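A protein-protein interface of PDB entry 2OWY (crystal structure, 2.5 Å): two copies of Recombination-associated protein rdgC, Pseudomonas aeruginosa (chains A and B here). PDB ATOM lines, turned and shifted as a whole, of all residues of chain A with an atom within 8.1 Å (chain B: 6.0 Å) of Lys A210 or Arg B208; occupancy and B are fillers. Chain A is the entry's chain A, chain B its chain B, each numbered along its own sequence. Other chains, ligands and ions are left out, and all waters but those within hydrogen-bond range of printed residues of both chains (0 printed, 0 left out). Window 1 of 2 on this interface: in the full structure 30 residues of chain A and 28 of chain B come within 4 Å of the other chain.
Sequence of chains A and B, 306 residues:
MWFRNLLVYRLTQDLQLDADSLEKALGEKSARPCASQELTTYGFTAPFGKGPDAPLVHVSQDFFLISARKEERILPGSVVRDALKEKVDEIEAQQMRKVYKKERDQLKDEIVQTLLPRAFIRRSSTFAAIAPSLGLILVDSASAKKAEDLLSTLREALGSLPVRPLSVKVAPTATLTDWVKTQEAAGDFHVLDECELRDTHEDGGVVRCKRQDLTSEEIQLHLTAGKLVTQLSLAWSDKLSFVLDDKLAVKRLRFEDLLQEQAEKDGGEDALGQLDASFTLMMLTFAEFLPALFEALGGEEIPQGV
N of Arg A208 sits at hydrogen-bond distance from O of Arg B208 (2.7 Å). O of Arg B208 sits close to O of Val A206, 3.4 Å away. NH1 of Arg A211 is in hydrogen-bond range of O of Gly B204 (2.5 Å). The backbone NH (N) of Lys A210 lies within hydrogen-bond range of the backbone carbonyl oxygen (O) of Val B206, 3.0 Å away. O of Val A206 is in hydrogen-bond range of N of Lys B210 (2.8 Å).
Among the printed residues, pairs that only touch across the chains: Val A207 with Arg B208, Gly A205 with Lys B210, Arg A211 with Gly B205, Arg A208 with Val B207, Cys A209 with Val B206, Val A206 with Cys B209, Gln A212 with Val B207, Arg A208 with Val B206, Lys A210 with Gly B205, Arg A211 with Val B206, Lys A210 with Arg B208, Val A207 with Val B207 and Arg A208 with Lys B210.
Gly A205 touches Lys B210, and with the chains exchanged Lys A210 touches Gly B205. Val A206 touches Arg B208, and with the chains exchanged Arg A208 touches Val B206. Arg A208 touches its own counterpart, Arg B208. Arg A208 touches Lys B210, and with the chains exchanged Lys A210 touches Arg B208.
Of chain B, only Gly B205 (3.6 Å), Val B206 (3.0 Å) and Arg B208 (3.7 Å) come within 4 Å of Lys A210. Of chain A, only Val A206 (3.4 Å), Val A207 (3.1 Å), Arg A208 (2.7 Å) and Lys A210 (3.7 Å) come within 4 Å of Arg B208. Printed residues of chain B within 4 Å of Val A206: Arg B208, Cys B209 and Lys B210. Of the printed residues of chain A, Lys B210 touches Gly A205, Val A206 and Arg A208. Of the printed residues of chain B, Val A207 touches Val B207 (3.7 Å) and Arg B208 (3.1 Å). Of the printed residues of chain A, Cys B209 touches Val A206. The nearest residue of chain A that does not touch Arg B208 is Cys A209 (4.9 Å).
Hydrophobic or aromatic side chains of chain B within 4 Å of the printed part of chain A: Val B206 and Val B207. Of the 20 printed residues of chain A, 8 touch a printed residue of chain B. Hydrophobic or aromatic side chains of chain A within 4 Å of the printed part of chain B: Val A207.
O of Asp A193 is in hydrogen-bond range of N of Arg A211 (2.9 Å). OE1 of Glu B196 is in salt-bridge range of NE of Arg B208 (2.9 Å). The backbone carbonyl oxygen (O) of Asp A193 sits at hydrogen-bond distance from the backbone NH (N) of Gln A212, 3.1 Å away. The backbone carbonyl oxygen (O) of Cys A195 lies within hydrogen-bond range of the backbone NH (N) of Cys A209. The backbone carbonyl oxygen (O) of Val A207 is in hydrogen-bond range of the backbone NH (N) of Leu A197 (2.8 Å). O of Val B207 is in hydrogen-bond range of N of Leu B197, 2.8 Å away.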
ATOM      1  N   ASP A 193      -6.216  19.387  26.493  1.00  0.00           N
ATOM      2  CA  ASP A 193      -6.780  19.316  25.139  1.00  0.00           C
ATOM      3  C   ASP A 193      -8.095  18.568  24.992  1.00  0.00           C
ATOM      4  O   ASP A 193      -8.331  17.898  23.990  1.00  0.00           O
ATOM      5  CB  ASP A 193      -5.751  18.682  24.202  1.00  0.00           C
ATOM      6  CG  ASP A 193      -5.326  17.287  24.663  1.00  0.00           C
ATOM      7  OD1 ASP A 193      -5.904  16.793  25.657  1.00  0.00           O
ATOM      8  OD2 ASP A 193      -4.419  16.687  24.031  1.00  0.00           O
ATOM      9  N   GLU A 194      -8.970  18.700  25.970  1.00  0.00           N
ATOM     10  CA  GLU A 194     -10.214  17.984  25.899  1.00  0.00           C
ATOM     11  C   GLU A 194     -11.301  18.713  26.660  1.00  0.00           C
ATOM     12  O   GLU A 194     -11.057  19.292  27.718  1.00  0.00           O
ATOM     13  CB  GLU A 194      -9.981  16.605  26.482  1.00  0.00           C
ATOM     14  CG  GLU A 194     -11.095  15.636  26.312  1.00  0.00           C
ATOM     15  CD  GLU A 194     -10.699  14.258  26.807  1.00  0.00           C
ATOM     16  OE1 GLU A 194     -11.606  13.415  26.990  1.00  0.00           O
ATOM     17  OE2 GLU A 194      -9.482  14.020  27.009  1.00  0.00           O
ATOM     18  N   CYS A 195     -12.507  18.696  26.117  1.00  0.00           N
ATOM     19  CA  CYS A 195     -13.605  19.357  26.790  1.00  0.00           C
ATOM     20  C   CYS A 195     -14.940  18.959  26.217  1.00  0.00           C
ATOM     21  O   CYS A 195     -15.028  18.343  25.151  1.00  0.00           O
ATOM     22  CB  CYS A 195     -13.464  20.879  26.688  1.00  0.00           C
ATOM     23  SG  CYS A 195     -13.874  21.525  25.068  1.00  0.00           S
ATOM     24  N   GLU A 196     -15.989  19.291  26.957  1.00  0.00           N
ATOM     25  CA  GLU A 196     -17.335  19.023  26.498  1.00  0.00           C
ATOM     26  C   GLU A 196     -18.050  20.358  26.549  1.00  0.00           C
ATOM     27  O   GLU A 196     -18.029  21.049  27.571  1.00  0.00           O
ATOM     28  CB  GLU A 196     -18.044  18.012  27.382  1.00  0.00           C
ATOM     29  CG  GLU A 196     -19.465  17.766  26.918  1.00  0.00           C
ATOM     30  CD  GLU A 196     -20.162  16.672  27.678  1.00  0.00           C
ATOM     31  OE1 GLU A 196     -19.695  15.510  27.627  1.00  0.00           O
ATOM     32  OE2 GLU A 196     -21.179  16.980  28.325  1.00  0.00           O
ATOM     33  N   LEU A 197     -18.663  20.724  25.432  1.00  0.00           N
ATOM     34  CA  LEU A 197     -19.368  21.988  25.330  1.00  0.00           C
ATOM     35  C   LEU A 197     -20.849  21.734  25.106  1.00  0.00           C
ATOM     36  O   LEU A 197     -21.219  20.755  24.453  1.00  0.00           O
ATOM     37  CB  LEU A 197     -18.802  22.809  24.164  1.00  0.00           C
ATOM     38  CG  LEU A 197     -17.303  23.150  24.161  1.00  0.00           C
ATOM     39  CD1 LEU A 197     -17.002  24.059  22.978  1.00  0.00           C
ATOM     40  CD2 LEU A 197     -16.899  23.829  25.461  1.00  0.00           C
ATOM     41  N   GLY A 205     -27.515  21.708  21.760  1.00  0.00           N
ATOM     42  CA  GLY A 205     -26.500  20.759  21.372  1.00  0.00           C
ATOM     43  C   GLY A 205     -25.362  20.442  22.320  1.00  0.00           C
ATOM     44  O   GLY A 205     -25.225  21.008  23.412  1.00  0.00           O
ATOM     45  N   VAL A 206     -24.544  19.497  21.868  1.00  0.00           N
ATOM     46  CA  VAL A 206     -23.382  19.061  22.603  1.00  0.00           C
ATOM     47  C   VAL A 206     -22.234  18.816  21.641  1.00  0.00           C
ATOM     48  O   VAL A 206     -22.371  18.121  20.632  1.00  0.00           O
ATOM     49  CB  VAL A 206     -23.665  17.785  23.373  1.00  0.00           C
ATOM     50  CG1 VAL A 206     -22.440  17.392  24.179  1.00  0.00           C
ATOM     51  CG2 VAL A 206     -24.856  18.003  24.286  1.00  0.00           C
ATOM     52  N   VAL A 207     -21.097  19.412  21.959  1.00  0.00           N
ATOM     53  CA  VAL A 207     -19.904  19.267  21.150  1.00  0.00           C
ATOM     54  C   VAL A 207     -18.793  18.675  22.021  1.00  0.00           C
ATOM     55  O   VAL A 207     -18.387  19.282  23.015  1.00  0.00           O
ATOM     56  CB  VAL A 207     -19.483  20.638  20.579  1.00  0.00           C
ATOM     57  CG1 VAL A 207     -18.126  20.555  19.956  1.00  0.00           C
ATOM     58  CG2 VAL A 207     -20.512  21.104  19.545  1.00  0.00           C
ATOM     59  N   ARG A 208     -18.318  17.485  21.672  1.00  0.00           N
ATOM     60  CA  ARG A 208     -17.247  16.874  22.460  1.00  0.00           C
ATOM     61  C   ARG A 208     -15.925  16.866  21.694  1.00  0.00           C
ATOM     62  O   ARG A 208     -15.839  16.328  20.591  1.00  0.00           O
ATOM     63  CB  ARG A 208     -17.625  15.451  22.874  1.00  0.00           C
ATOM     64  CG  ARG A 208     -18.863  15.364  23.752  1.00  0.00           C
ATOM     65  CD  ARG A 208     -19.011  13.972  24.355  1.00  0.00           C
ATOM     66  NE  ARG A 208     -19.115  12.915  23.344  1.00  0.00           N
ATOM     67  CZ  ARG A 208     -20.247  12.568  22.733  1.00  0.00           C
ATOM     68  NH1 ARG A 208     -21.384  13.201  23.036  1.00  0.00           N
ATOM     69  NH2 ARG A 208     -20.249  11.581  21.833  1.00  0.00           N
ATOM     70  N   CYS A 209     -14.898  17.468  22.286  1.00  0.00           N
ATOM     71  CA  CYS A 209     -13.584  17.562  21.651  1.00  0.00           C
ATOM     72  C   CYS A 209     -12.495  16.807  22.408  1.00  0.00           C
ATOM     73  O   CYS A 209     -12.469  16.813  23.630  1.00  0.00           O
ATOM     74  CB  CYS A 209     -13.161  19.031  21.536  1.00  0.00           C
ATOM     75  SG  CYS A 209     -14.506  20.223  21.201  1.00  0.00           S
ATOM     76  N   LYS A 210     -11.599  16.145  21.676  1.00  0.00           N
ATOM     77  CA  LYS A 210     -10.486  15.440  22.295  1.00  0.00           C
ATOM     78  C   LYS A 210      -9.279  15.628  21.396  1.00  0.00           C
ATOM     79  O   LYS A 210      -9.418  15.710  20.180  1.00  0.00           O
ATOM     80  CB  LYS A 210     -10.810  13.959  22.516  1.00  0.00           C
ATOM     81  CG  LYS A 210     -10.863  13.058  21.296  1.00  0.00           C
ATOM     82  CD  LYS A 210     -11.041  11.595  21.762  1.00  0.00           C
ATOM     83  CE  LYS A 210     -11.320  10.605  20.612  1.00  0.00           C
ATOM     84  NZ  LYS A 210     -11.705   9.244  21.124  1.00  0.00           N
ATOM     85  N   ARG A 211      -8.100  15.737  22.001  1.00  0.00           N
ATOM     86  CA  ARG A 211      -6.861  15.964  21.263  1.00  0.00           C
ATOM     87  C   ARG A 211      -6.996  17.222  20.417  1.00  0.00           C
ATOM     88  O   ARG A 211      -6.558  17.273  19.274  1.00  0.00           O
ATOM     89  CB  ARG A 211      -6.528  14.762  20.374  1.00  0.00           C
ATOM     90  CG  ARG A 211      -6.061  13.536  21.147  1.00  0.00           C
ATOM     91  CD  ARG A 211      -5.755  12.382  20.224  1.00  0.00           C
ATOM     92  NE  ARG A 211      -6.743  11.317  20.363  1.00  0.00           N
ATOM     93  CZ  ARG A 211      -7.521  10.891  19.377  1.00  0.00           C
ATOM     94  NH1 ARG A 211      -7.427  11.441  18.178  1.00  0.00           N
ATOM     95  NH2 ARG A 211      -8.396   9.919  19.590  1.00  0.00           N
ATOM     96  N   GLN A 212      -7.603  18.245  21.005  1.00  0.00           N
ATOM     97  CA  GLN A 212      -7.821  19.514  20.330  1.00  0.00           C
ATOM     98  C   GLN A 212      -7.223  20.677  21.089  1.00  0.00           C
ATOM     99  O   GLN A 212      -7.269  20.715  22.317  1.00  0.00           O
ATOM    100  CB  GLN A 212      -9.318  19.743  20.150  1.00  0.00           C
ATOM    101  CG  GLN A 212      -9.830  19.453  18.750  1.00  0.00           C
ATOM    102  CD  GLN A 212      -9.921  20.708  17.897  1.00  0.00           C
ATOM    103  OE1 GLN A 212     -10.740  20.776  16.985  1.00  0.00           O
ATOM    104  NE2 GLN A 212      -9.085  21.712  18.190  1.00  0.00           N
ATOM    105  N   ASP A 213      -6.651  21.622  20.354  1.00  0.00           N
ATOM    106  CA  ASP A 213      -6.059  22.819  20.959  1.00  0.00           C
ATOM    107  C   ASP A 213      -7.248  23.715  21.311  1.00  0.00           C
ATOM    108  O   ASP A 213      -7.935  24.223  20.427  1.00  0.00           O
ATOM    109  CB  ASP A 213      -5.133  23.516  19.954  1.00  0.00           C
ATOM    110  CG  ASP A 213      -4.508  24.796  20.498  1.00  0.00           C
ATOM    111  OD1 ASP A 213      -3.771  25.454  19.732  1.00  0.00           O
ATOM    112  OD2 ASP A 213      -4.746  25.149  21.679  1.00  0.00           O
ATOM    113  N   LEU A 214      -7.490  23.893  22.603  1.00  0.00           N
ATOM    114  CA  LEU A 214      -8.626  24.686  23.061  1.00  0.00           C
ATOM    115  C   LEU A 214      -8.462  26.194  22.898  1.00  0.00           C
ATOM    116  O   LEU A 214      -9.353  26.968  23.245  1.00  0.00           O
ATOM    117  CB  LEU A 214      -8.954  24.303  24.510  1.00  0.00           C
ATOM    118  CG  LEU A 214      -9.868  23.077  24.720  1.00  0.00           C
ATOM    119  CD1 LEU A 214      -9.839  22.125  23.536  1.00  0.00           C
ATOM    120  CD2 LEU A 214      -9.450  22.368  25.982  1.00  0.00           C
ATOM    121  N   ILE A 219     -12.884  26.518  18.880  1.00  0.00           N
ATOM    122  CA  ILE A 219     -13.422  26.426  20.233  1.00  0.00           C
ATOM    123  C   ILE A 219     -13.932  27.783  20.677  1.00  0.00           C
ATOM    124  O   ILE A 219     -15.001  27.887  21.289  1.00  0.00           O
ATOM    125  CB  ILE A 219     -12.352  25.906  21.230  1.00  0.00           C
ATOM    126  CG1 ILE A 219     -11.785  24.575  20.728  1.00  0.00           C
ATOM    127  CG2 ILE A 219     -12.962  25.700  22.608  1.00  0.00           C
ATOM    128  CD1 ILE A 219     -12.840  23.537  20.395  1.00  0.00           C
ATOM    129  N   HIS A 222     -17.295  28.576  19.263  1.00  0.00           N
ATOM    130  CA  HIS A 222     -18.355  27.814  19.927  1.00  0.00           C
ATOM    131  C   HIS A 222     -18.809  28.534  21.194  1.00  0.00           C
ATOM    132  O   HIS A 222     -19.999  28.591  21.497  1.00  0.00           O
ATOM    133  CB  HIS A 222     -17.865  26.433  20.326  1.00  0.00           C
ATOM    134  CG  HIS A 222     -18.060  25.398  19.272  1.00  0.00           C
ATOM    135  ND1 HIS A 222     -19.303  25.070  18.778  1.00  0.00           N
ATOM    136  CD2 HIS A 222     -17.171  24.643  18.589  1.00  0.00           C
ATOM    137  CE1 HIS A 222     -19.173  24.161  17.831  1.00  0.00           C
ATOM    138  NE2 HIS A 222     -17.888  23.885  17.696  1.00  0.00           N
ATOM    139  N   LYS A 227     -21.974  28.267  23.747  1.00  0.00           N
ATOM    140  CA  LYS A 227     -21.693  26.992  24.407  1.00  0.00           C
ATOM    141  C   LYS A 227     -21.055  27.211  25.767  1.00  0.00           C
ATOM    142  O   LYS A 227     -20.321  28.180  25.980  1.00  0.00           O
ATOM    143  CB  LYS A 227     -20.753  26.123  23.567  1.00  0.00           C
ATOM    144  CG  LYS A 227     -21.315  25.659  22.231  1.00  0.00           C
ATOM    145  CD  LYS A 227     -22.374  24.572  22.400  1.00  0.00           C
ATOM    146  CE  LYS A 227     -22.654  23.877  21.074  1.00  0.00           C
ATOM    147  NZ  LYS A 227     -22.998  24.821  19.971  1.00  0.00           N
ATOM    148  N   SER A 233     -10.551  18.920  30.692  1.00  0.00           N
ATOM    149  CA  SER A 233      -9.367  18.136  31.015  1.00  0.00           C
ATOM    150  C   SER A 233      -8.355  19.131  31.571  1.00  0.00           C
ATOM    151  O   SER A 233      -8.071  20.148  30.924  1.00  0.00           O
ATOM    152  CB  SER A 233      -8.827  17.472  29.752  1.00  0.00           C
ATOM    153  OG  SER A 233      -7.572  16.887  29.999  1.00  0.00           O
ATOM    154  N   ARG A 252     -10.872  10.641  35.764  1.00  0.00           N
ATOM    155  CA  ARG A 252      -9.645  10.208  35.102  1.00  0.00           C
ATOM    156  C   ARG A 252      -8.410  10.765  35.817  1.00  0.00           C
ATOM    157  O   ARG A 252      -7.498  11.326  35.197  1.00  0.00           O
ATOM    158  CB  ARG A 252      -9.676  10.664  33.642  1.00  0.00           C
ATOM    159  CG  ARG A 252      -8.842   9.805  32.699  1.00  0.00           C
ATOM    160  CD  ARG A 252      -8.556  10.512  31.374  1.00  0.00           C
ATOM    161  NE  ARG A 252      -9.763  10.816  30.605  1.00  0.00           N
ATOM    162  CZ  ARG A 252      -9.796  11.677  29.588  1.00  0.00           C
ATOM    163  NH1 ARG A 252     -10.932  11.895  28.941  1.00  0.00           N
ATOM    164  NH2 ARG A 252      -8.696  12.331  29.226  1.00  0.00           N
ATOM    165  N   CYS B 195     -22.756  14.753  13.554  1.00  0.00           N
ATOM    166  CA  CYS B 195     -21.596  14.377  12.759  1.00  0.00           C
ATOM    167  C   CYS B 195     -20.363  14.210  13.627  1.00  0.00           C
ATOM    168  O   CYS B 195     -20.382  14.512  14.820  1.00  0.00           O
ATOM    169  CB  CYS B 195     -21.307  15.450  11.712  1.00  0.00           C
ATOM    170  SG  CYS B 195     -20.676  16.966  12.434  1.00  0.00           S
ATOM    171  N   GLU B 196     -19.295  13.718  13.005  1.00  0.00           N
ATOM    172  CA  GLU B 196     -18.017  13.531  13.670  1.00  0.00           C
ATOM    173  C   GLU B 196     -16.942  14.094  12.755  1.00  0.00           C
ATOM    174  O   GLU B 196     -16.756  13.624  11.635  1.00  0.00           O
ATOM    175  CB  GLU B 196     -17.735  12.053  13.938  1.00  0.00           C
ATOM    176  CG  GLU B 196     -16.332  11.810  14.492  1.00  0.00           C
ATOM    177  CD  GLU B 196     -16.102  10.377  14.965  1.00  0.00           C
ATOM    178  OE1 GLU B 196     -16.849   9.930  15.872  1.00  0.00           O
ATOM    179  OE2 GLU B 196     -15.174   9.703  14.440  1.00  0.00           O
ATOM    180  N   LEU B 197     -16.243  15.114  13.231  1.00  0.00           N
ATOM    181  CA  LEU B 197     -15.201  15.738  12.441  1.00  0.00           C
ATOM    182  C   LEU B 197     -13.847  15.304  12.975  1.00  0.00           C
ATOM    183  O   LEU B 197     -13.685  15.116  14.180  1.00  0.00           O
ATOM    184  CB  LEU B 197     -15.329  17.253  12.537  1.00  0.00           C
ATOM    185  CG  LEU B 197     -16.738  17.804  12.322  1.00  0.00           C
ATOM    186  CD1 LEU B 197     -16.774  19.264  12.704  1.00  0.00           C
ATOM    187  CD2 LEU B 197     -17.159  17.594  10.880  1.00  0.00           C
ATOM    188  N   ARG B 198     -12.865  15.127  12.098  1.00  0.00           N
ATOM    189  CA  ARG B 198     -11.553  14.745  12.601  1.00  0.00           C
ATOM    190  C   ARG B 198     -10.355  15.018  11.709  1.00  0.00           C
ATOM    191  O   ARG B 198     -10.430  14.975  10.487  1.00  0.00           O
ATOM    192  CB  ARG B 198     -11.549  13.280  13.036  1.00  0.00           C
ATOM    193  CG  ARG B 198     -11.784  12.273  11.969  1.00  0.00           C
ATOM    194  CD  ARG B 198     -11.420  10.890  12.511  1.00  0.00           C
ATOM    195  NE  ARG B 198     -12.322  10.430  13.560  1.00  0.00           N
ATOM    196  CZ  ARG B 198     -11.936   9.747  14.637  1.00  0.00           C
ATOM    197  NH1 ARG B 198     -10.656   9.452  14.811  1.00  0.00           N
ATOM    198  NH2 ARG B 198     -12.833   9.349  15.537  1.00  0.00           N
ATOM    199  N   GLY B 204      -4.673  12.847  15.692  1.00  0.00           N
ATOM    200  CA  GLY B 204      -5.283  14.117  15.360  1.00  0.00           C
ATOM    201  C   GLY B 204      -6.489  14.429  16.225  1.00  0.00           C
ATOM    202  O   GLY B 204      -6.918  13.613  17.039  1.00  0.00           O
ATOM    203  N   GLY B 205      -7.041  15.622  16.048  1.00  0.00           N
ATOM    204  CA  GLY B 205      -8.192  16.013  16.840  1.00  0.00           C
ATOM    205  C   GLY B 205      -9.478  15.306  16.460  1.00  0.00           C
ATOM    206  O   GLY B 205      -9.606  14.742  15.372  1.00  0.00           O
ATOM    207  N   VAL B 206     -10.430  15.304  17.381  1.00  0.00           N
ATOM    208  CA  VAL B 206     -11.725  14.712  17.108  1.00  0.00           C
ATOM    209  C   VAL B 206     -12.804  15.556  17.767  1.00  0.00           C
ATOM    210  O   VAL B 206     -12.712  15.864  18.946  1.00  0.00           O
ATOM    211  CB  VAL B 206     -11.798  13.271  17.610  1.00  0.00           C
ATOM    212  CG1 VAL B 206     -13.138  12.663  17.229  1.00  0.00           C
ATOM    213  CG2 VAL B 206     -10.654  12.457  16.992  1.00  0.00           C
ATOM    214  N   VAL B 207     -13.804  15.948  16.982  1.00  0.00           N
ATOM    215  CA  VAL B 207     -14.922  16.760  17.456  1.00  0.00           C
ATOM    216  C   VAL B 207     -16.238  16.067  17.126  1.00  0.00           C
ATOM    217  O   VAL B 207     -16.486  15.722  15.968  1.00  0.00           O
ATOM    218  CB  VAL B 207     -14.951  18.145  16.777  1.00  0.00           C
ATOM    219  CG1 VAL B 207     -16.182  18.923  17.239  1.00  0.00           C
ATOM    220  CG2 VAL B 207     -13.687  18.918  17.109  1.00  0.00           C
ATOM    221  N   ARG B 208     -17.078  15.868  18.143  1.00  0.00           N
ATOM    222  CA  ARG B 208     -18.374  15.223  17.952  1.00  0.00           C
ATOM    223  C   ARG B 208     -19.507  16.176  18.254  1.00  0.00           C
ATOM    224  O   ARG B 208     -19.544  16.806  19.318  1.00  0.00           O
ATOM    225  CB  ARG B 208     -18.509  13.986  18.832  1.00  0.00           C
ATOM    226  CG  ARG B 208     -17.490  12.947  18.526  1.00  0.00           C
ATOM    227  CD  ARG B 208     -17.939  11.571  18.937  1.00  0.00           C
ATOM    228  NE  ARG B 208     -16.843  10.642  18.701  1.00  0.00           N
ATOM    229  CZ  ARG B 208     -15.731  10.611  19.427  1.00  0.00           C
ATOM    230  NH1 ARG B 208     -15.589  11.457  20.447  1.00  0.00           N
ATOM    231  NH2 ARG B 208     -14.751   9.763  19.115  1.00  0.00           N
ATOM    232  N   CYS B 209     -20.442  16.246  17.312  1.00  0.00           N
ATOM    233  CA  CYS B 209     -21.582  17.138  17.403  1.00  0.00           C
ATOM    234  C   CYS B 209     -22.937  16.449  17.490  1.00  0.00           C
ATOM    235  O   CYS B 209     -23.282  15.645  16.630  1.00  0.00           O
ATOM    236  CB  CYS B 209     -21.587  18.080  16.187  1.00  0.00           C
ATOM    237  SG  CYS B 209     -20.087  19.082  15.992  1.00  0.00           S
ATOM    238  N   LYS B 210     -23.696  16.771  18.537  1.00  0.00           N
ATOM    239  CA  LYS B 210     -25.045  16.240  18.724  1.00  0.00           C
ATOM    240  C   LYS B 210     -26.002  17.419  18.755  1.00  0.00           C
ATOM    241  O   LYS B 210     -25.687  18.461  19.321  1.00  0.00           O
ATOM    242  CB  LYS B 210     -25.176  15.465  20.032  1.00  0.00           C
ATOM    243  CG  LYS B 210     -24.966  13.972  19.905  1.00  0.00           C
ATOM    244  CD  LYS B 210     -25.226  13.295  21.250  1.00  0.00           C
ATOM    245  CE  LYS B 210     -24.621  11.890  21.324  1.00  0.00           C
ATOM    246  NZ  LYS B 210     -24.621  11.369  22.732  1.00  0.00           N
ATOM    247  N   GLN B 231     -18.311  11.099  10.066  1.00  0.00           N
ATOM    248  CA  GLN B 231     -19.621  10.561  10.443  1.00  0.00           C
ATOM    249  C   GLN B 231     -20.645  11.655  10.199  1.00  0.00           C
ATOM    250  O   GLN B 231     -20.387  12.818  10.509  1.00  0.00           O
ATOM    251  CB  GLN B 231     -19.657  10.132  11.908  1.00  0.00           C
ATOM    252  CG  GLN B 231     -18.927   8.834  12.179  1.00  0.00           C
ATOM    253  CD  GLN B 231     -19.495   8.097  13.374  1.00  0.00           C
ATOM    254  OE1 GLN B 231     -20.709   7.949  13.502  1.00  0.00           O
ATOM    255  NE2 GLN B 231     -18.621   7.619  14.249  1.00  0.00           N
